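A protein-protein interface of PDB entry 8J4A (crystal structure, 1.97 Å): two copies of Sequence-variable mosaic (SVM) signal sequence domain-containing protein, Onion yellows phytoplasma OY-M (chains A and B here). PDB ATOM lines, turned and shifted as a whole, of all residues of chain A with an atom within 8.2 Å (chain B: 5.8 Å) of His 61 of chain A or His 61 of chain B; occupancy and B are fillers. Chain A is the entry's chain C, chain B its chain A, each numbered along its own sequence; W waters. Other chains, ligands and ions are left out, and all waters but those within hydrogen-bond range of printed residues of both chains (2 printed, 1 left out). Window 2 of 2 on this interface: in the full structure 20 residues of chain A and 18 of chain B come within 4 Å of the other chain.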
ATOM      1  N   PRO A  41       4.351 -21.852   2.636  1.00  0.00           N
ATOM      2  CA  PRO A  41       3.775 -21.931   1.286  1.00  0.00           C
ATOM      3  C   PRO A  41       2.624 -22.924   1.179  1.00  0.00           C
ATOM      4  O   PRO A  41       2.609 -23.989   1.812  1.00  0.00           O
ATOM      5  CB  PRO A  41       4.970 -22.353   0.419  1.00  0.00           C
ATOM      6  CG  PRO A  41       5.865 -23.081   1.366  1.00  0.00           C
ATOM      7  CD  PRO A  41       5.722 -22.389   2.688  1.00  0.00           C
ATOM      8  N   ASN A  58       7.231 -30.178   4.054  1.00  0.00           N
ATOM      9  CA  ASN A  58       8.677 -29.976   3.980  1.00  0.00           C
ATOM     10  C   ASN A  58       9.103 -29.133   2.767  1.00  0.00           C
ATOM     11  O   ASN A  58       9.910 -29.580   1.957  1.00  0.00           O
ATOM     12  CB  ASN A  58       9.413 -31.310   3.987  1.00  0.00           C
ATOM     13  CG  ASN A  58       9.252 -32.040   5.290  1.00  0.00           C
ATOM     14  OD1 ASN A  58       9.120 -31.419   6.353  1.00  0.00           O
ATOM     15  ND2 ASN A  58       9.242 -33.368   5.223  1.00  0.00           N
ATOM     16  N   PRO A  59       8.606 -27.892   2.660  1.00  0.00           N
ATOM     17  CA  PRO A  59       8.913 -27.090   1.479  1.00  0.00           C
ATOM     18  C   PRO A  59      10.336 -26.570   1.522  1.00  0.00           C
ATOM     19  O   PRO A  59      10.884 -26.304   2.606  1.00  0.00           O
ATOM     20  CB  PRO A  59       7.900 -25.934   1.568  1.00  0.00           C
ATOM     21  CG  PRO A  59       7.669 -25.766   3.061  1.00  0.00           C
ATOM     22  CD  PRO A  59       7.781 -27.165   3.647  1.00  0.00           C
ATOM     23  N   PRO A  60      10.984 -26.412   0.365  1.00  0.00           N
ATOM     24  CA  PRO A  60      12.181 -25.562   0.307  1.00  0.00           C
ATOM     25  C   PRO A  60      11.823 -24.185   0.833  1.00  0.00           C
ATOM     26  O   PRO A  60      10.704 -23.705   0.643  1.00  0.00           O
ATOM     27  CB  PRO A  60      12.546 -25.528  -1.188  1.00  0.00           C
ATOM     28  CG  PRO A  60      11.510 -26.296  -1.910  1.00  0.00           C
ATOM     29  CD  PRO A  60      10.659 -27.047  -0.928  1.00  0.00           C
ATOM     30  N   HIS A  61      12.742 -23.539   1.540  1.00  0.00           N
ATOM     31  CA  HIS A  61      12.254 -22.287   2.090  1.00  0.00           C
ATOM     32  C   HIS A  61      12.523 -21.104   1.178  1.00  0.00           C
ATOM     33  O   HIS A  61      12.351 -19.958   1.605  1.00  0.00           O
ATOM     34  CB  HIS A  61      12.744 -22.067   3.524  1.00  0.00           C
ATOM     35  CG  HIS A  61      14.197 -21.767   3.660  1.00  0.00           C
ATOM     36  ND1 HIS A  61      14.740 -20.534   3.369  1.00  0.00           N
ATOM     37  CD2 HIS A  61      15.211 -22.523   4.141  1.00  0.00           C
ATOM     38  CE1 HIS A  61      16.036 -20.557   3.624  1.00  0.00           C
ATOM     39  NE2 HIS A  61      16.344 -21.751   4.099  1.00  0.00           N
ATOM     40  N   ASN A  62      12.849 -21.348  -0.094  1.00  0.00           N
ATOM     41  CA  ASN A  62      12.591 -20.335  -1.114  1.00  0.00           C
ATOM     42  C   ASN A  62      11.314 -20.617  -1.918  1.00  0.00           C
ATOM     43  O   ASN A  62      11.048 -19.924  -2.901  1.00  0.00           O
ATOM     44  CB  ASN A  62      13.784 -20.188  -2.051  1.00  0.00           C
ATOM     45  CG  ASN A  62      13.918 -21.345  -2.993  1.00  0.00           C
ATOM     46  OD1 ASN A  62      13.770 -22.501  -2.589  1.00  0.00           O
ATOM     47  ND2 ASN A  62      14.188 -21.051  -4.264  1.00  0.00           N
ATOM     48  N   LEU A  63      10.496 -21.581  -1.501  1.00  0.00           N
ATOM     49  CA  LEU A  63       9.198 -21.791  -2.136  1.00  0.00           C
ATOM     50  C   LEU A  63       8.158 -20.828  -1.549  1.00  0.00           C
ATOM     51  O   LEU A  63       8.069 -20.653  -0.326  1.00  0.00           O
ATOM     52  CB  LEU A  63       8.743 -23.240  -1.965  1.00  0.00           C
ATOM     53  CG  LEU A  63       7.356 -23.589  -2.514  1.00  0.00           C
ATOM     54  CD1 LEU A  63       7.358 -23.501  -4.025  1.00  0.00           C
ATOM     55  CD2 LEU A  63       6.928 -24.961  -2.070  1.00  0.00           C
ATOM     56  N   LEU A  64       7.389 -20.184  -2.427  1.00  0.00           N
ATOM     57  CA  LEU A  64       6.351 -19.262  -1.977  1.00  0.00           C
ATOM     58  C   LEU A  64       4.951 -19.843  -2.076  1.00  0.00           C
ATOM     59  O   LEU A  64       4.096 -19.483  -1.264  1.00  0.00           O
ATOM     60  CB  LEU A  64       6.391 -17.960  -2.782  1.00  0.00           C
ATOM     61  CG  LEU A  64       7.614 -17.062  -2.665  1.00  0.00           C
ATOM     62  CD1 LEU A  64       7.400 -15.838  -3.511  1.00  0.00           C
ATOM     63  CD2 LEU A  64       7.861 -16.684  -1.205  1.00  0.00           C
ATOM     64  N   TRP A  99       8.497 -18.864  -6.579  1.00  0.00           N
ATOM     65  CA  TRP A  99       9.753 -18.974  -5.858  1.00  0.00           C
ATOM     66  C   TRP A  99      10.208 -17.595  -5.395  1.00  0.00           C
ATOM     67  O   TRP A  99       9.997 -16.592  -6.078  1.00  0.00           O
ATOM     68  CB  TRP A  99      10.840 -19.582  -6.746  1.00  0.00           C
ATOM     69  CG  TRP A  99      10.580 -20.954  -7.249  1.00  0.00           C
ATOM     70  CD1 TRP A  99      10.126 -21.303  -8.500  1.00  0.00           C
ATOM     71  CD2 TRP A  99      10.794 -22.183  -6.544  1.00  0.00           C
ATOM     72  NE1 TRP A  99      10.036 -22.674  -8.599  1.00  0.00           N
ATOM     73  CE2 TRP A  99      10.446 -23.235  -7.417  1.00  0.00           C
ATOM     74  CE3 TRP A  99      11.237 -22.497  -5.255  1.00  0.00           C
ATOM     75  CZ2 TRP A  99      10.536 -24.572  -7.043  1.00  0.00           C
ATOM     76  CZ3 TRP A  99      11.319 -23.818  -4.893  1.00  0.00           C
ATOM     77  CH2 TRP A  99      10.970 -24.840  -5.777  1.00  0.00           C
ATOM     78  N   GLN A 100      10.867 -17.563  -4.241  1.00  0.00           N
ATOM     79  CA  GLN A 100      11.496 -16.346  -3.743  1.00  0.00           C
ATOM     80  C   GLN A 100      12.934 -16.278  -4.244  1.00  0.00           C
ATOM     81  O   GLN A 100      13.699 -17.230  -4.074  1.00  0.00           O
ATOM     82  CB  GLN A 100      11.463 -16.316  -2.214  1.00  0.00           C
ATOM     83  CG  GLN A 100      12.075 -15.063  -1.607  1.00  0.00           C
ATOM     84  CD  GLN A 100      11.091 -14.296  -0.767  1.00  0.00           C
ATOM     85  OE1 GLN A 100       9.886 -14.365  -0.982  1.00  0.00           O
ATOM     86  NE2 GLN A 100      11.597 -13.556   0.202  1.00  0.00           N
ATOM     87  N   TYR A 101      13.299 -15.154  -4.849  1.00  0.00           N
ATOM     88  CA  TYR A 101      14.663 -14.962  -5.320  1.00  0.00           C
ATOM     89  C   TYR A 101      15.613 -14.736  -4.153  1.00  0.00           C
ATOM     90  O   TYR A 101      15.310 -13.962  -3.241  1.00  0.00           O
ATOM     91  CB  TYR A 101      14.740 -13.759  -6.262  1.00  0.00           C
ATOM     92  CG  TYR A 101      16.075 -13.577  -6.981  1.00  0.00           C
ATOM     93  CD1 TYR A 101      17.216 -13.165  -6.299  1.00  0.00           C
ATOM     94  CD2 TYR A 101      16.173 -13.769  -8.350  1.00  0.00           C
ATOM     95  CE1 TYR A 101      18.420 -12.997  -6.945  1.00  0.00           C
ATOM     96  CE2 TYR A 101      17.371 -13.583  -9.013  1.00  0.00           C
ATOM     97  CZ  TYR A 101      18.486 -13.197  -8.308  1.00  0.00           C
ATOM     98  OH  TYR A 101      19.678 -13.016  -8.975  1.00  0.00           O
ATOM     99  N   GLU A 102      16.752 -15.430  -4.191  1.00  0.00           N
ATOM    100  CA  GLU A 102      18.019 -14.900  -3.671  1.00  0.00           C
ATOM    101  C   GLU A 102      19.160 -15.918  -3.750  1.00  0.00           C
ATOM    102  O   GLU A 102      20.342 -15.553  -3.697  1.00  0.00           O
ATOM    103  CB  GLU A 102      17.862 -14.395  -2.240  1.00  0.00           C
ATOM    104  CG  GLU A 102      18.870 -13.336  -1.909  1.00  0.00           C
ATOM    105  CD  GLU A 102      20.281 -13.933  -1.779  1.00  0.00           C
ATOM    106  OE1 GLU A 102      20.442 -14.924  -1.036  1.00  0.00           O
ATOM    107  OE2 GLU A 102      21.185 -13.393  -2.409  1.00  0.00           O
ATOM    108  N   PRO B  59      22.491 -18.472  -5.476  1.00  0.00           N
ATOM    109  CA  PRO B  59      21.856 -19.789  -5.560  1.00  0.00           C
ATOM    110  C   PRO B  59      20.721 -19.932  -4.558  1.00  0.00           C
ATOM    111  O   PRO B  59      20.761 -19.337  -3.468  1.00  0.00           O
ATOM    112  CB  PRO B  59      23.003 -20.756  -5.223  1.00  0.00           C
ATOM    113  CG  PRO B  59      23.920 -19.952  -4.351  1.00  0.00           C
ATOM    114  CD  PRO B  59      23.795 -18.513  -4.776  1.00  0.00           C
ATOM    115  N   PRO B  60      19.707 -20.750  -4.868  1.00  0.00           N
ATOM    116  CA  PRO B  60      18.732 -21.117  -3.838  1.00  0.00           C
ATOM    117  C   PRO B  60      19.445 -21.725  -2.642  1.00  0.00           C
ATOM    118  O   PRO B  60      20.482 -22.383  -2.782  1.00  0.00           O
ATOM    119  CB  PRO B  60      17.824 -22.135  -4.541  1.00  0.00           C
ATOM    120  CG  PRO B  60      17.917 -21.782  -5.987  1.00  0.00           C
ATOM    121  CD  PRO B  60      19.357 -21.318  -6.185  1.00  0.00           C
ATOM    122  N   HIS B  61      18.881 -21.485  -1.454  1.00  0.00           N
ATOM    123  CA  HIS B  61      19.492 -21.957  -0.214  1.00  0.00           C
ATOM    124  C   HIS B  61      19.743 -23.460  -0.218  1.00  0.00           C
ATOM    125  O   HIS B  61      20.714 -23.925   0.392  1.00  0.00           O
ATOM    126  CB  HIS B  61      18.612 -21.591   0.980  1.00  0.00           C
ATOM    127  CG  HIS B  61      19.290 -21.778   2.302  1.00  0.00           C
ATOM    128  ND1 HIS B  61      18.775 -22.583   3.296  1.00  0.00           N
ATOM    129  CD2 HIS B  61      20.449 -21.276   2.789  1.00  0.00           C
ATOM    130  CE1 HIS B  61      19.580 -22.557   4.344  1.00  0.00           C
ATOM    131  NE2 HIS B  61      20.606 -21.773   4.061  1.00  0.00           N
ATOM    132  N   ASN B  62      18.905 -24.236  -0.901  1.00  0.00           N
ATOM    133  CA  ASN B  62      19.054 -25.688  -0.882  1.00  0.00           C
ATOM    134  C   ASN B  62      19.732 -26.255  -2.127  1.00  0.00           C
ATOM    135  O   ASN B  62      19.732 -27.476  -2.303  1.00  0.00           O
ATOM    136  CB  ASN B  62      17.697 -26.358  -0.693  1.00  0.00           C
ATOM    137  CG  ASN B  62      16.722 -26.027  -1.800  1.00  0.00           C
ATOM    138  OD1 ASN B  62      16.719 -24.916  -2.342  1.00  0.00           O
ATOM    139  ND2 ASN B  62      15.878 -26.996  -2.145  1.00  0.00           N
ATOM    140  N   LEU B  63      20.293 -25.418  -2.995  1.00  0.00           N
ATOM    141  CA  LEU B  63      21.054 -25.927  -4.131  1.00  0.00           C
ATOM    142  C   LEU B  63      22.408 -26.427  -3.644  1.00  0.00           C
ATOM    143  O   LEU B  63      23.102 -25.717  -2.920  1.00  0.00           O
ATOM    144  CB  LEU B  63      21.272 -24.842  -5.177  1.00  0.00           C
ATOM    145  CG  LEU B  63      22.007 -25.337  -6.408  1.00  0.00           C
ATOM    146  CD1 LEU B  63      21.164 -26.401  -7.099  1.00  0.00           C
ATOM    147  CD2 LEU B  63      22.368 -24.200  -7.368  1.00  0.00           C
ATOM    148  N   GLU B 102      14.856 -30.190   2.710  1.00  0.00           N
ATOM    149  CA  GLU B 102      14.739 -29.325   3.884  1.00  0.00           C
ATOM    150  C   GLU B 102      13.582 -29.739   4.783  1.00  0.00           C
ATOM    151  O   GLU B 102      13.777 -30.508   5.727  1.00  0.00           O
ATOM    152  CB  GLU B 102      14.589 -27.867   3.449  1.00  0.00           C
ATOM    153  CG  GLU B 102      15.930 -27.179   3.190  1.00  0.00           C
ATOM    154  CD  GLU B 102      15.871 -26.214   2.028  1.00  0.00           C
ATOM    155  OE1 GLU B 102      15.015 -26.413   1.136  1.00  0.00           O
ATOM    156  OE2 GLU B 102      16.681 -25.259   2.002  1.00  0.00           O
HETATM  157  O   HOH W   1      14.475 -24.572  -4.223  1.00  0.00           O
HETATM  158  O   HOH W   2      12.439 -30.029   0.951  1.00  0.00           O
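ND1 of His 61 of chain B is in hydrogen-bond range of NE2 of His 61 of chain A (2.7 Å).
O of Asn 62 of chain A lies within hydrogen-bond range of N of Gln 100 of chain A (2.7 Å).
The side-chain amide nitrogen of Asn 62 of chain B sits close to the side-chain carboxylate of Glu 102 of chain B, 3.4 Å away.
Asn 62 of chain B touches Pro 60 of chain A.
Glu 102 of chain B touches Pro 60 of chain A (OE1 to CA, 3.1 Å).
Glu 102 of chain B touches His 61 of chain A.
Pro 60 of chain B touches Asn 62 of chain A (CB to ND2, 3.8 Å).
Asn 62 of chain A touches Asn 62 of chain B.
Glu 102 of chain A touches Pro 59 of chain B.
Printed residues of chain A within 4 Å of Pro 60 of chain B: Asn 62.
Of the printed residues of chain A, Glu 102 of chain B touches Pro 60 (3.1 Å) and His 61 (3.7 Å).
Of the printed residues of chain B, Glu 102 of chain A touches Pro 59 (3.8 Å).
Printed residues of chain B within 4 Å of Asn 62 of chain A: Pro 60 (3.8 Å) and Asn 62 (3.8 Å).
Printed residues of chain A within 4 Å of Asn 62 of chain B: Pro 60 (3.8 Å) and Asn 62 (3.8 Å).
The nearest residue of chain B that does not touch His 61 of chain A is Asn 62 of chain B (5.7 Å).
Hydrophobic or aromatic side chains of chain B that line the printed part of chain A: Pro 60 and His 61.
Printed residues of chain A that touch a printed residue of chain B: Pro 60, His 61, Asn 62 and Glu 102.
Hydrophobic or aromatic side chains of chain A that line the printed part of chain B: Pro 60 and His 61.
Among the printed residues, 7 pairs touch across the chains.
Among the printed residues, no Asp or Glu carboxylate lies within 4 Å of a Lys or Arg side-chain nitrogen of the other chain.
Pro 60 of chain A touches Asn 62 of chain B, and with the chains exchanged Asn 62 of chain A touches Pro 60 of chain B.
His 61 of chain A touches its own counterpart, His 61 of chain B.
Asn 62 of chain B touches its own counterpart, Asn 62 of chain A.
Glu 102 of chain A touches Pro 59 of chain B, but with the chains exchanged Pro 59 of chain A does not touch Glu 102 of chain B (4.1 Å).
Water W1 bridges OD1 of Asn 62 of chain A (2.7 Å) and OD1 of Asn 62 of chain B (2.9 Å).
Water W2 bridges the backbone carbonyl oxygen of Asn 58 of chain A (2.8 Å) and the backbone NH of Glu 102 of chain B (3.0 Å).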
